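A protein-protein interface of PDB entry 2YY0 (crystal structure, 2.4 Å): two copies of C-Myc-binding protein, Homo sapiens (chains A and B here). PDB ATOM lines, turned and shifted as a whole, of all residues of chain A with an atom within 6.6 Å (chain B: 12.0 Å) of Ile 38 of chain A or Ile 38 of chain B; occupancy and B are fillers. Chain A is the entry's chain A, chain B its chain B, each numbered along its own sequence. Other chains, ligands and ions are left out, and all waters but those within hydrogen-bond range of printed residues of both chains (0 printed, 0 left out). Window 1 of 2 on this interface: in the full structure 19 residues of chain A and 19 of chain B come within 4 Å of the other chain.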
ATOM      1  N   GLU A  33     -16.474 -20.345 -17.404  1.00  0.00           N
ATOM      2  CA  GLU A  33     -17.553 -19.851 -16.563  1.00  0.00           C
ATOM      3  C   GLU A  33     -18.873 -20.184 -17.244  1.00  0.00           C
ATOM      4  O   GLU A  33     -19.847 -20.531 -16.581  1.00  0.00           O
ATOM      5  CB  GLU A  33     -17.432 -18.340 -16.373  1.00  0.00           C
ATOM      6  CG  GLU A  33     -18.474 -17.729 -15.441  1.00  0.00           C
ATOM      7  CD  GLU A  33     -18.664 -16.229 -15.681  1.00  0.00           C
ATOM      8  OE1 GLU A  33     -19.036 -15.855 -16.821  1.00  0.00           O
ATOM      9  OE2 GLU A  33     -18.447 -15.426 -14.740  1.00  0.00           O
ATOM     10  N   LYS A  34     -18.913 -20.076 -18.567  1.00  0.00           N
ATOM     11  CA  LYS A  34     -20.133 -20.404 -19.299  1.00  0.00           C
ATOM     12  C   LYS A  34     -20.370 -21.909 -19.204  1.00  0.00           C
ATOM     13  O   LYS A  34     -21.501 -22.381 -19.253  1.00  0.00           O
ATOM     14  CB  LYS A  34     -20.015 -20.023 -20.775  1.00  0.00           C
ATOM     15  CG  LYS A  34     -20.155 -18.540 -21.077  1.00  0.00           C
ATOM     16  CD  LYS A  34     -19.862 -18.246 -22.550  1.00  0.00           C
ATOM     17  CE  LYS A  34     -20.770 -19.043 -23.480  1.00  0.00           C
ATOM     18  NZ  LYS A  34     -20.413 -18.857 -24.918  1.00  0.00           N
ATOM     19  N   TYR A  35     -19.298 -22.664 -19.052  1.00  0.00           N
ATOM     20  CA  TYR A  35     -19.432 -24.100 -18.974  1.00  0.00           C
ATOM     21  C   TYR A  35     -19.860 -24.574 -17.609  1.00  0.00           C
ATOM     22  O   TYR A  35     -20.601 -25.542 -17.499  1.00  0.00           O
ATOM     23  CB  TYR A  35     -18.125 -24.765 -19.380  1.00  0.00           C
ATOM     24  CG  TYR A  35     -18.075 -26.233 -19.067  1.00  0.00           C
ATOM     25  CD1 TYR A  35     -17.612 -26.681 -17.829  1.00  0.00           C
ATOM     26  CD2 TYR A  35     -18.478 -27.176 -20.005  1.00  0.00           C
ATOM     27  CE1 TYR A  35     -17.546 -28.030 -17.538  1.00  0.00           C
ATOM     28  CE2 TYR A  35     -18.414 -28.530 -19.725  1.00  0.00           C
ATOM     29  CZ  TYR A  35     -17.946 -28.950 -18.494  1.00  0.00           C
ATOM     30  OH  TYR A  35     -17.849 -30.296 -18.217  1.00  0.00           O
ATOM     31  N   GLU A  36     -19.385 -23.903 -16.567  1.00  0.00           N
ATOM     32  CA  GLU A  36     -19.754 -24.268 -15.196  1.00  0.00           C
ATOM     33  C   GLU A  36     -21.210 -23.901 -14.897  1.00  0.00           C
ATOM     34  O   GLU A  36     -21.799 -24.391 -13.937  1.00  0.00           O
ATOM     35  CB  GLU A  36     -18.845 -23.561 -14.183  1.00  0.00           C
ATOM     36  CG  GLU A  36     -17.456 -24.164 -14.038  1.00  0.00           C
ATOM     37  CD  GLU A  36     -17.496 -25.618 -13.607  1.00  0.00           C
ATOM     38  OE1 GLU A  36     -18.284 -25.948 -12.689  1.00  0.00           O
ATOM     39  OE2 GLU A  36     -16.733 -26.425 -14.179  1.00  0.00           O
ATOM     40  N   ALA A  37     -21.787 -23.040 -15.724  1.00  0.00           N
ATOM     41  CA  ALA A  37     -23.164 -22.611 -15.535  1.00  0.00           C
ATOM     42  C   ALA A  37     -24.155 -23.639 -16.078  1.00  0.00           C
ATOM     43  O   ALA A  37     -25.244 -23.808 -15.535  1.00  0.00           O
ATOM     44  CB  ALA A  37     -23.388 -21.261 -16.205  1.00  0.00           C
ATOM     45  N   ILE A  38     -23.784 -24.319 -17.156  1.00  0.00           N
ATOM     46  CA  ILE A  38     -24.666 -25.324 -17.725  1.00  0.00           C
ATOM     47  C   ILE A  38     -24.526 -26.569 -16.862  1.00  0.00           C
ATOM     48  O   ILE A  38     -25.506 -27.266 -16.613  1.00  0.00           O
ATOM     49  CB  ILE A  38     -24.293 -25.664 -19.188  1.00  0.00           C
ATOM     50  CG1 ILE A  38     -24.280 -24.397 -20.040  1.00  0.00           C
ATOM     51  CG2 ILE A  38     -25.307 -26.634 -19.766  1.00  0.00           C
ATOM     52  CD1 ILE A  38     -25.578 -23.616 -19.991  1.00  0.00           C
ATOM     53  N   VAL A  39     -23.303 -26.837 -16.401  1.00  0.00           N
ATOM     54  CA  VAL A  39     -23.051 -27.990 -15.540  1.00  0.00           C
ATOM     55  C   VAL A  39     -23.944 -27.823 -14.324  1.00  0.00           C
ATOM     56  O   VAL A  39     -24.463 -28.791 -13.783  1.00  0.00           O
ATOM     57  CB  VAL A  39     -21.589 -28.048 -15.029  1.00  0.00           C
ATOM     58  CG1 VAL A  39     -21.455 -29.141 -13.975  1.00  0.00           C
ATOM     59  CG2 VAL A  39     -20.627 -28.310 -16.174  1.00  0.00           C
ATOM     60  N   GLU A  40     -24.102 -26.573 -13.902  1.00  0.00           N
ATOM     61  CA  GLU A  40     -24.918 -26.235 -12.750  1.00  0.00           C
ATOM     62  C   GLU A  40     -26.376 -26.218 -13.175  1.00  0.00           C
ATOM     63  O   GLU A  40     -27.265 -26.583 -12.411  1.00  0.00           O
ATOM     64  CB  GLU A  40     -24.511 -24.860 -12.210  1.00  0.00           C
ATOM     65  CG  GLU A  40     -25.241 -24.449 -10.949  1.00  0.00           C
ATOM     66  CD  GLU A  40     -25.287 -25.562  -9.924  1.00  0.00           C
ATOM     67  OE1 GLU A  40     -24.242 -26.212  -9.697  1.00  0.00           O
ATOM     68  OE2 GLU A  40     -26.368 -25.785  -9.341  1.00  0.00           O
ATOM     69  N   GLU A  41     -26.606 -25.791 -14.409  1.00  0.00           N
ATOM     70  CA  GLU A  41     -27.950 -25.719 -14.953  1.00  0.00           C
ATOM     71  C   GLU A  41     -28.562 -27.120 -15.051  1.00  0.00           C
ATOM     72  O   GLU A  41     -29.729 -27.324 -14.712  1.00  0.00           O
ATOM     73  CB  GLU A  41     -27.903 -25.052 -16.328  1.00  0.00           C
ATOM     74  CG  GLU A  41     -29.248 -24.645 -16.893  1.00  0.00           C
ATOM     75  CD  GLU A  41     -29.103 -23.824 -18.161  1.00  0.00           C
ATOM     76  OE1 GLU A  41     -28.482 -22.737 -18.101  1.00  0.00           O
ATOM     77  OE2 GLU A  41     -29.607 -24.268 -19.218  1.00  0.00           O
ATOM     78  N   ASN A  42     -27.772 -28.087 -15.504  1.00  0.00           N
ATOM     79  CA  ASN A  42     -28.256 -29.453 -15.623  1.00  0.00           C
ATOM     80  C   ASN A  42     -28.472 -30.081 -14.250  1.00  0.00           C
ATOM     81  O   ASN A  42     -29.370 -30.902 -14.074  1.00  0.00           O
ATOM     82  CB  ASN A  42     -27.275 -30.304 -16.428  1.00  0.00           C
ATOM     83  CG  ASN A  42     -27.035 -29.752 -17.816  1.00  0.00           C
ATOM     84  OD1 ASN A  42     -27.919 -29.135 -18.421  1.00  0.00           O
ATOM     85  ND2 ASN A  42     -25.838 -29.986 -18.341  1.00  0.00           N
ATOM     86  N   LYS A  43     -27.646 -29.702 -13.282  1.00  0.00           N
ATOM     87  CA  LYS A  43     -27.771 -30.224 -11.926  1.00  0.00           C
ATOM     88  C   LYS A  43     -29.221 -30.038 -11.500  1.00  0.00           C
ATOM     89  O   LYS A  43     -29.867 -30.970 -11.029  1.00  0.00           O
ATOM     90  CB  LYS A  43     -26.848 -29.454 -10.971  1.00  0.00           C
ATOM     91  CG  LYS A  43     -26.937 -29.879  -9.504  1.00  0.00           C
ATOM     92  CD  LYS A  43     -26.103 -28.955  -8.616  1.00  0.00           C
ATOM     93  CE  LYS A  43     -26.085 -29.411  -7.160  1.00  0.00           C
ATOM     94  NZ  LYS A  43     -25.389 -30.717  -6.982  1.00  0.00           N
ATOM     95  N   ALA B  29      -9.989 -24.083 -27.468  1.00  0.00           N
ATOM     96  CA  ALA B  29     -10.677 -25.034 -28.361  1.00  0.00           C
ATOM     97  C   ALA B  29     -11.221 -26.220 -27.581  1.00  0.00           C
ATOM     98  O   ALA B  29     -12.339 -26.640 -27.771  1.00  0.00           O
ATOM     99  CB  ALA B  29      -9.718 -25.551 -29.424  1.00  0.00           C
ATOM    100  N   GLU B  30     -10.402 -26.768 -26.703  1.00  0.00           N
ATOM    101  CA  GLU B  30     -10.783 -27.908 -25.884  1.00  0.00           C
ATOM    102  C   GLU B  30     -12.002 -27.568 -24.990  1.00  0.00           C
ATOM    103  O   GLU B  30     -13.004 -28.306 -24.945  1.00  0.00           O
ATOM    104  CB  GLU B  30      -9.571 -28.284 -25.032  1.00  0.00           C
ATOM    105  CG  GLU B  30      -9.553 -29.692 -24.510  1.00  0.00           C
ATOM    106  CD  GLU B  30     -10.715 -29.948 -23.614  1.00  0.00           C
ATOM    107  OE1 GLU B  30     -10.859 -29.179 -22.641  1.00  0.00           O
ATOM    108  OE2 GLU B  30     -11.483 -30.903 -23.887  1.00  0.00           O
ATOM    109  N   MET B  31     -11.918 -26.441 -24.289  1.00  0.00           N
ATOM    110  CA  MET B  31     -12.991 -26.004 -23.398  1.00  0.00           C
ATOM    111  C   MET B  31     -14.273 -25.781 -24.194  1.00  0.00           C
ATOM    112  O   MET B  31     -15.355 -26.129 -23.736  1.00  0.00           O
ATOM    113  CB  MET B  31     -12.573 -24.715 -22.680  1.00  0.00           C
ATOM    114  CG  MET B  31     -13.572 -24.194 -21.624  1.00  0.00           C
ATOM    115  SD  MET B  31     -14.006 -25.395 -20.313  1.00  0.00           S
ATOM    116  CE  MET B  31     -12.498 -26.251 -20.087  1.00  0.00           C
ATOM    117  N   LYS B  32     -14.150 -25.213 -25.393  1.00  0.00           N
ATOM    118  CA  LYS B  32     -15.312 -24.970 -26.230  1.00  0.00           C
ATOM    119  C   LYS B  32     -15.940 -26.297 -26.660  1.00  0.00           C
ATOM    120  O   LYS B  32     -17.155 -26.399 -26.819  1.00  0.00           O
ATOM    121  CB  LYS B  32     -14.907 -24.170 -27.459  1.00  0.00           C
ATOM    122  CG  LYS B  32     -16.084 -23.672 -28.278  1.00  0.00           C
ATOM    123  CD  LYS B  32     -15.638 -22.827 -29.449  1.00  0.00           C
ATOM    124  CE  LYS B  32     -16.843 -22.307 -30.219  1.00  0.00           C
ATOM    125  NZ  LYS B  32     -17.711 -23.424 -30.682  1.00  0.00           N
ATOM    126  N   GLU B  33     -15.110 -27.315 -26.859  1.00  0.00           N
ATOM    127  CA  GLU B  33     -15.619 -28.622 -27.236  1.00  0.00           C
ATOM    128  C   GLU B  33     -16.493 -29.131 -26.105  1.00  0.00           C
ATOM    129  O   GLU B  33     -17.617 -29.537 -26.334  1.00  0.00           O
ATOM    130  CB  GLU B  33     -14.476 -29.615 -27.450  1.00  0.00           C
ATOM    131  CG  GLU B  33     -13.765 -29.502 -28.780  1.00  0.00           C
ATOM    132  CD  GLU B  33     -14.359 -30.419 -29.835  1.00  0.00           C
ATOM    133  OE1 GLU B  33     -15.577 -30.306 -30.093  1.00  0.00           O
ATOM    134  OE2 GLU B  33     -13.610 -31.252 -30.402  1.00  0.00           O
ATOM    135  N   LYS B  34     -15.969 -29.106 -24.882  1.00  0.00           N
ATOM    136  CA  LYS B  34     -16.711 -29.597 -23.727  1.00  0.00           C
ATOM    137  C   LYS B  34     -18.001 -28.838 -23.488  1.00  0.00           C
ATOM    138  O   LYS B  34     -19.027 -29.425 -23.163  1.00  0.00           O
ATOM    139  CB  LYS B  34     -15.854 -29.543 -22.453  1.00  0.00           C
ATOM    140  CG  LYS B  34     -14.859 -30.696 -22.315  1.00  0.00           C
ATOM    141  CD  LYS B  34     -14.399 -30.907 -20.859  1.00  0.00           C
ATOM    142  CE  LYS B  34     -13.726 -29.666 -20.283  1.00  0.00           C
ATOM    143  NZ  LYS B  34     -13.585 -29.718 -18.792  1.00  0.00           N
ATOM    144  N   TYR B  35     -17.939 -27.525 -23.648  1.00  0.00           N
ATOM    145  CA  TYR B  35     -19.100 -26.679 -23.449  1.00  0.00           C
ATOM    146  C   TYR B  35     -20.229 -27.030 -24.413  1.00  0.00           C
ATOM    147  O   TYR B  35     -21.378 -27.192 -24.006  1.00  0.00           O
ATOM    148  CB  TYR B  35     -18.703 -25.219 -23.632  1.00  0.00           C
ATOM    149  CG  TYR B  35     -19.873 -24.299 -23.760  1.00  0.00           C
ATOM    150  CD1 TYR B  35     -20.526 -23.805 -22.629  1.00  0.00           C
ATOM    151  CD2 TYR B  35     -20.337 -23.919 -25.021  1.00  0.00           C
ATOM    152  CE1 TYR B  35     -21.611 -22.947 -22.753  1.00  0.00           C
ATOM    153  CE2 TYR B  35     -21.418 -23.068 -25.159  1.00  0.00           C
ATOM    154  CZ  TYR B  35     -22.053 -22.582 -24.021  1.00  0.00           C
ATOM    155  OH  TYR B  35     -23.129 -21.731 -24.166  1.00  0.00           O
ATOM    156  N   GLU B  36     -19.907 -27.127 -25.692  1.00  0.00           N
ATOM    157  CA  GLU B  36     -20.913 -27.464 -26.694  1.00  0.00           C
ATOM    158  C   GLU B  36     -21.542 -28.857 -26.454  1.00  0.00           C
ATOM    159  O   GLU B  36     -22.696 -29.093 -26.798  1.00  0.00           O
ATOM    160  CB  GLU B  36     -20.292 -27.400 -28.100  1.00  0.00           C
ATOM    161  CG  GLU B  36     -19.786 -26.010 -28.528  1.00  0.00           C
ATOM    162  CD  GLU B  36     -20.908 -24.995 -28.770  1.00  0.00           C
ATOM    163  OE1 GLU B  36     -20.599 -23.832 -29.123  1.00  0.00           O
ATOM    164  OE2 GLU B  36     -22.095 -25.354 -28.611  1.00  0.00           O
ATOM    165  N   ALA B  37     -20.788 -29.780 -25.868  1.00  0.00           N
ATOM    166  CA  ALA B  37     -21.326 -31.112 -25.603  1.00  0.00           C
ATOM    167  C   ALA B  37     -22.436 -31.004 -24.566  1.00  0.00           C
ATOM    168  O   ALA B  37     -23.530 -31.537 -24.741  1.00  0.00           O
ATOM    169  CB  ALA B  37     -20.238 -32.036 -25.080  1.00  0.00           C
ATOM    170  N   ILE B  38     -22.134 -30.307 -23.483  1.00  0.00           N
ATOM    171  CA  ILE B  38     -23.068 -30.133 -22.392  1.00  0.00           C
ATOM    172  C   ILE B  38     -24.272 -29.300 -22.810  1.00  0.00           C
ATOM    173  O   ILE B  38     -25.338 -29.378 -22.206  1.00  0.00           O
ATOM    174  CB  ILE B  38     -22.360 -29.478 -21.197  1.00  0.00           C
ATOM    175  CG1 ILE B  38     -22.888 -30.074 -19.897  1.00  0.00           C
ATOM    176  CG2 ILE B  38     -22.565 -27.965 -21.228  1.00  0.00           C
ATOM    177  CD1 ILE B  38     -22.096 -29.649 -18.674  1.00  0.00           C
ATOM    178  N   VAL B  39     -24.109 -28.483 -23.840  1.00  0.00           N
ATOM    179  CA  VAL B  39     -25.231 -27.684 -24.298  1.00  0.00           C
ATOM    180  C   VAL B  39     -26.202 -28.654 -24.954  1.00  0.00           C
ATOM    181  O   VAL B  39     -27.414 -28.462 -24.905  1.00  0.00           O
ATOM    182  CB  VAL B  39     -24.783 -26.615 -25.313  1.00  0.00           C
ATOM    183  CG1 VAL B  39     -26.008 -25.937 -25.960  1.00  0.00           C
ATOM    184  CG2 VAL B  39     -23.932 -25.581 -24.605  1.00  0.00           C
ATOM    185  N   GLU B  40     -25.659 -29.705 -25.564  1.00  0.00           N
ATOM    186  CA  GLU B  40     -26.473 -30.729 -26.213  1.00  0.00           C
ATOM    187  C   GLU B  40     -27.249 -31.482 -25.140  1.00  0.00           C
ATOM    188  O   GLU B  40     -28.462 -31.656 -25.243  1.00  0.00           O
ATOM    189  CB  GLU B  40     -25.588 -31.701 -26.995  1.00  0.00           C
ATOM    190  CG  GLU B  40     -25.031 -31.123 -28.283  1.00  0.00           C
ATOM    191  CD  GLU B  40     -26.111 -30.863 -29.323  1.00  0.00           C
ATOM    192  OE1 GLU B  40     -26.486 -31.815 -30.043  1.00  0.00           O
ATOM    193  OE2 GLU B  40     -26.592 -29.709 -29.412  1.00  0.00           O
ATOM    194  N   GLU B  41     -26.544 -31.913 -24.102  1.00  0.00           N
ATOM    195  CA  GLU B  41     -27.185 -32.631 -23.025  1.00  0.00           C
ATOM    196  C   GLU B  41     -28.225 -31.731 -22.367  1.00  0.00           C
ATOM    197  O   GLU B  41     -29.358 -32.141 -22.127  1.00  0.00           O
ATOM    198  CB  GLU B  41     -26.145 -33.087 -21.997  1.00  0.00           C
ATOM    199  CG  GLU B  41     -26.305 -34.546 -21.608  1.00  0.00           C
ATOM    200  CD  GLU B  41     -27.700 -34.859 -21.080  1.00  0.00           C
ATOM    201  OE1 GLU B  41     -27.968 -34.591 -19.888  1.00  0.00           O
ATOM    202  OE2 GLU B  41     -28.532 -35.365 -21.864  1.00  0.00           O
ATOM    203  N   ASN B  42     -27.836 -30.492 -22.087  1.00  0.00           N
ATOM    204  CA  ASN B  42     -28.735 -29.537 -21.459  1.00  0.00           C
ATOM    205  C   ASN B  42     -30.017 -29.416 -22.268  1.00  0.00           C
ATOM    206  O   ASN B  42     -31.100 -29.290 -21.706  1.00  0.00           O
ATOM    207  CB  ASN B  42     -28.052 -28.169 -21.334  1.00  0.00           C
ATOM    208  CG  ASN B  42     -28.986 -27.087 -20.818  1.00  0.00           C
ATOM    209  OD1 ASN B  42     -29.382 -27.084 -19.648  1.00  0.00           O
ATOM    210  ND2 ASN B  42     -29.346 -26.161 -21.694  1.00  0.00           N
ATOM    211  N   LYS B  43     -29.904 -29.460 -23.590  1.00  0.00           N
ATOM    212  CA  LYS B  43     -31.089 -29.353 -24.417  1.00  0.00           C
ATOM    213  C   LYS B  43     -31.949 -30.615 -24.318  1.00  0.00           C
ATOM    214  O   LYS B  43     -33.177 -30.544 -24.425  1.00  0.00           O
ATOM    215  CB  LYS B  43     -30.706 -29.083 -25.875  1.00  0.00           C
ATOM    216  CG  LYS B  43     -29.925 -27.780 -26.073  1.00  0.00           C
ATOM    217  CD  LYS B  43     -30.033 -27.249 -27.494  1.00  0.00           C
ATOM    218  CE  LYS B  43     -29.614 -28.282 -28.517  1.00  0.00           C
ATOM    219  NZ  LYS B  43     -29.880 -27.795 -29.900  1.00  0.00           N
ATOM    220  N   LYS B  44     -31.312 -31.765 -24.106  1.00  0.00           N
ATOM    221  CA  LYS B  44     -32.053 -33.016 -23.986  1.00  0.00           C
ATOM    222  C   LYS B  44     -32.828 -33.055 -22.667  1.00  0.00           C
ATOM    223  O   LYS B  44     -33.997 -33.439 -22.640  1.00  0.00           O
ATOM    224  CB  LYS B  44     -31.108 -34.217 -24.089  1.00  0.00           C
ATOM    225  CG  LYS B  44     -30.548 -34.443 -25.498  1.00  0.00           C
ATOM    226  CD  LYS B  44     -29.693 -35.710 -25.574  1.00  0.00           C
ATOM    227  CE  LYS B  44     -29.080 -35.889 -26.957  1.00  0.00           C
ATOM    228  NZ  LYS B  44     -30.128 -35.850 -28.015  1.00  0.00           N
ATOM    229  N   LEU B  45     -32.177 -32.651 -21.581  1.00  0.00           N
ATOM    230  CA  LEU B  45     -32.828 -32.621 -20.288  1.00  0.00           C
ATOM    231  C   LEU B  45     -34.068 -31.752 -20.385  1.00  0.00           C
ATOM    232  O   LEU B  45     -35.124 -32.131 -19.888  1.00  0.00           O
ATOM    233  CB  LEU B  45     -31.891 -32.060 -19.221  1.00  0.00           C
ATOM    234  CG  LEU B  45     -30.683 -32.926 -18.848  1.00  0.00           C
ATOM    235  CD1 LEU B  45     -29.876 -32.220 -17.757  1.00  0.00           C
ATOM    236  CD2 LEU B  45     -31.152 -34.305 -18.372  1.00  0.00           C
ATOM    237  N   LYS B  46     -33.946 -30.593 -21.030  1.00  0.00           N
ATOM    238  CA  LYS B  46     -35.077 -29.669 -21.194  1.00  0.00           C
ATOM    239  C   LYS B  46     -36.224 -30.292 -21.992  1.00  0.00           C
ATOM    240  O   LYS B  46     -37.393 -30.019 -21.732  1.00  0.00           O
ATOM    241  CB  LYS B  46     -34.632 -28.378 -21.891  1.00  0.00           C
ATOM    242  CG  LYS B  46     -33.609 -27.553 -21.122  1.00  0.00           C
ATOM    243  CD  LYS B  46     -33.227 -26.297 -21.908  1.00  0.00           C
ATOM    244  CE  LYS B  46     -32.131 -25.512 -21.209  1.00  0.00           C
ATOM    245  NZ  LYS B  46     -32.513 -25.141 -19.822  1.00  0.00           N
ATOM    246  N   ALA B  47     -35.880 -31.115 -22.976  1.00  0.00           N
ATOM    247  CA  ALA B  47     -36.879 -31.791 -23.790  1.00  0.00           C
ATOM    248  C   ALA B  47     -37.671 -32.758 -22.904  1.00  0.00           C
ATOM    249  O   ALA B  47     -38.886 -32.875 -23.025  1.00  0.00           O
ATOM    250  CB  ALA B  47     -36.202 -32.547 -24.922  1.00  0.00           C
ATOM    251  N   LYS B  48     -36.977 -33.452 -22.008  1.00  0.00           N
ATOM    252  CA  LYS B  48     -37.646 -34.383 -21.114  1.00  0.00           C
ATOM    253  C   LYS B  48     -38.615 -33.671 -20.174  1.00  0.00           C
ATOM    254  O   LYS B  48     -39.763 -34.091 -20.030  1.00  0.00           O
ATOM    255  CB  LYS B  48     -36.624 -35.200 -20.320  1.00  0.00           C
ATOM    256  CG  LYS B  48     -36.083 -36.391 -21.101  1.00  0.00           C
ATOM    257  CD  LYS B  48     -35.269 -37.335 -20.230  1.00  0.00           C
ATOM    258  CE  LYS B  48     -33.933 -36.732 -19.816  1.00  0.00           C
ATOM    259  NZ  LYS B  48     -33.115 -37.684 -19.002  1.00  0.00           N
ATOM    260  N   LEU B  49     -38.168 -32.589 -19.546  1.00  0.00           N
ATOM    261  CA  LEU B  49     -39.042 -31.850 -18.651  1.00  0.00           C
ATOM    262  C   LEU B  49     -40.302 -31.364 -19.360  1.00  0.00           C
ATOM    263  O   LEU B  49     -41.363 -31.229 -18.747  1.00  0.00           O
ATOM    264  CB  LEU B  49     -38.311 -30.656 -18.046  1.00  0.00           C
ATOM    265  CG  LEU B  49     -37.588 -30.914 -16.725  1.00  0.00           C
ATOM    266  CD1 LEU B  49     -37.177 -29.568 -16.144  1.00  0.00           C
ATOM    267  CD2 LEU B  49     -38.495 -31.654 -15.735  1.00  0.00           C
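The side-chain amide oxygen (OD1) of Asn 42 of chain B lies close to the side-chain carboxylate (OE2) of Glu 41 of chain A, at 2.9 Å.
The side-chain amide oxygen (OD1) of Asn 42 of chain A lies close to the side-chain amide oxygen (OD1) of Asn 42 of chain B (2.8 Å).
OE2 of Glu 41 of chain A is in salt-bridge range of NZ of Lys 46 of chain B.
The backbone carbonyl oxygen (O) of Ile 38 of chain A lies close to the side-chain amide nitrogen (ND2) of Asn 42 of chain A, at 3.2 Å.
Tyr 35 of chain B touches Lys 34 of chain A.
Lys 34 of chain B touches Tyr 35 of chain A (O to CE2, 3.6 Å).
CD2 of Tyr 35 of chain A touches CA of Tyr 35 of chain B, at 3.5 Å.
Tyr 35 of chain A touches Ile 38 of chain B.
Ile 38 of chain A touches Ile 38 of chain B.
Asn 42 of chain B touches Ile 38 of chain A.
Val 39 of chain A touches Ile 38 of chain B (CG2 to CD1, 3.2 Å).
Ile 38 of chain B touches Asn 42 of chain A (CG1 to ND2, 3.3 Å).
Asn 42 of chain A touches Leu 45 of chain B (CB to CD1, 3.5 Å).
No residue of chain B comes within 4 Å of Glu 36 of chain A.
Of chain B, only Ile 38 (3.2 Å) comes within 4 Å of Val 39 of chain A.
No residue of chain B comes within 4 Å of Glu 40 of chain A.
Glu 41 of chain A touches just these residues of chain B: Asn 42 (2.9 Å) and Lys 46 (3.1 Å).
Asn 42 of chain A touches just these residues of chain B: Ile 38, Asn 42 and Leu 45.
Of the printed residues of chain A, Lys 34 of chain B touches Tyr 35.
Of the printed residues of chain A, Ile 38 of chain B touches Tyr 35, Ile 38, Val 39 and Asn 42.
Of the printed residues of chain A, Asn 42 of chain B touches Ile 38 (3.5 Å), Glu 41 (2.9 Å) and Asn 42 (2.8 Å).
Of the printed residues of chain A, Leu 45 of chain B touches Asn 42.
The nearest residue of chain B that does not touch Ile 38 of chain A is Tyr 35 of chain B (4.1 Å).
The nearest printed residue of chain A that does not touch Tyr 35 of chain B is Ile 38 of chain A (4.1 Å).
Of the 21 printed residues of chain B, 6 touch a printed residue of chain A.
Printed residues of chain B that touch a printed residue of chain A: Lys 34, Tyr 35, Ile 38, Asn 42, Leu 45 and Lys 46.
Hydrophobic or aromatic side chains of chain B within 4 Å of the printed part of chain A: Tyr 35, Ile 38 and Leu 45.
Of the 11 printed residues of chain A, 6 touch a printed residue of chain B.
Hydrophobic or aromatic side chains of chain A that line the printed part of chain B: Tyr 35, Ile 38 and Val 39.
Among the printed residues, 12 pairs touch across the chains.
Among the printed residues, Asp or Glu carboxylates within 4 Å of a Lys or Arg side-chain nitrogen of the other chain: Glu 41 of chain A with Lys 46 of chain B.
Lys 34 of chain A touches Tyr 35 of chain B, and with the chains exchanged Tyr 35 of chain A touches Lys 34 of chain B.
Tyr 35 of chain B touches its own counterpart, Tyr 35 of chain A.
Ile 38 of chain A touches its own counterpart, Ile 38 of chain B.
Ile 38 of chain A touches Asn 42 of chain B, and with the chains exchanged Asn 42 of chain A touches Ile 38 of chain B.
Positions printed for both chains: 33, 34, 35, 36, 37, 38, 39, 40, 41, 42 and 43.
Of the 12 pairs that touch across the chains among the printed residues, 7 have their exchanged pair printed and touching as well.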
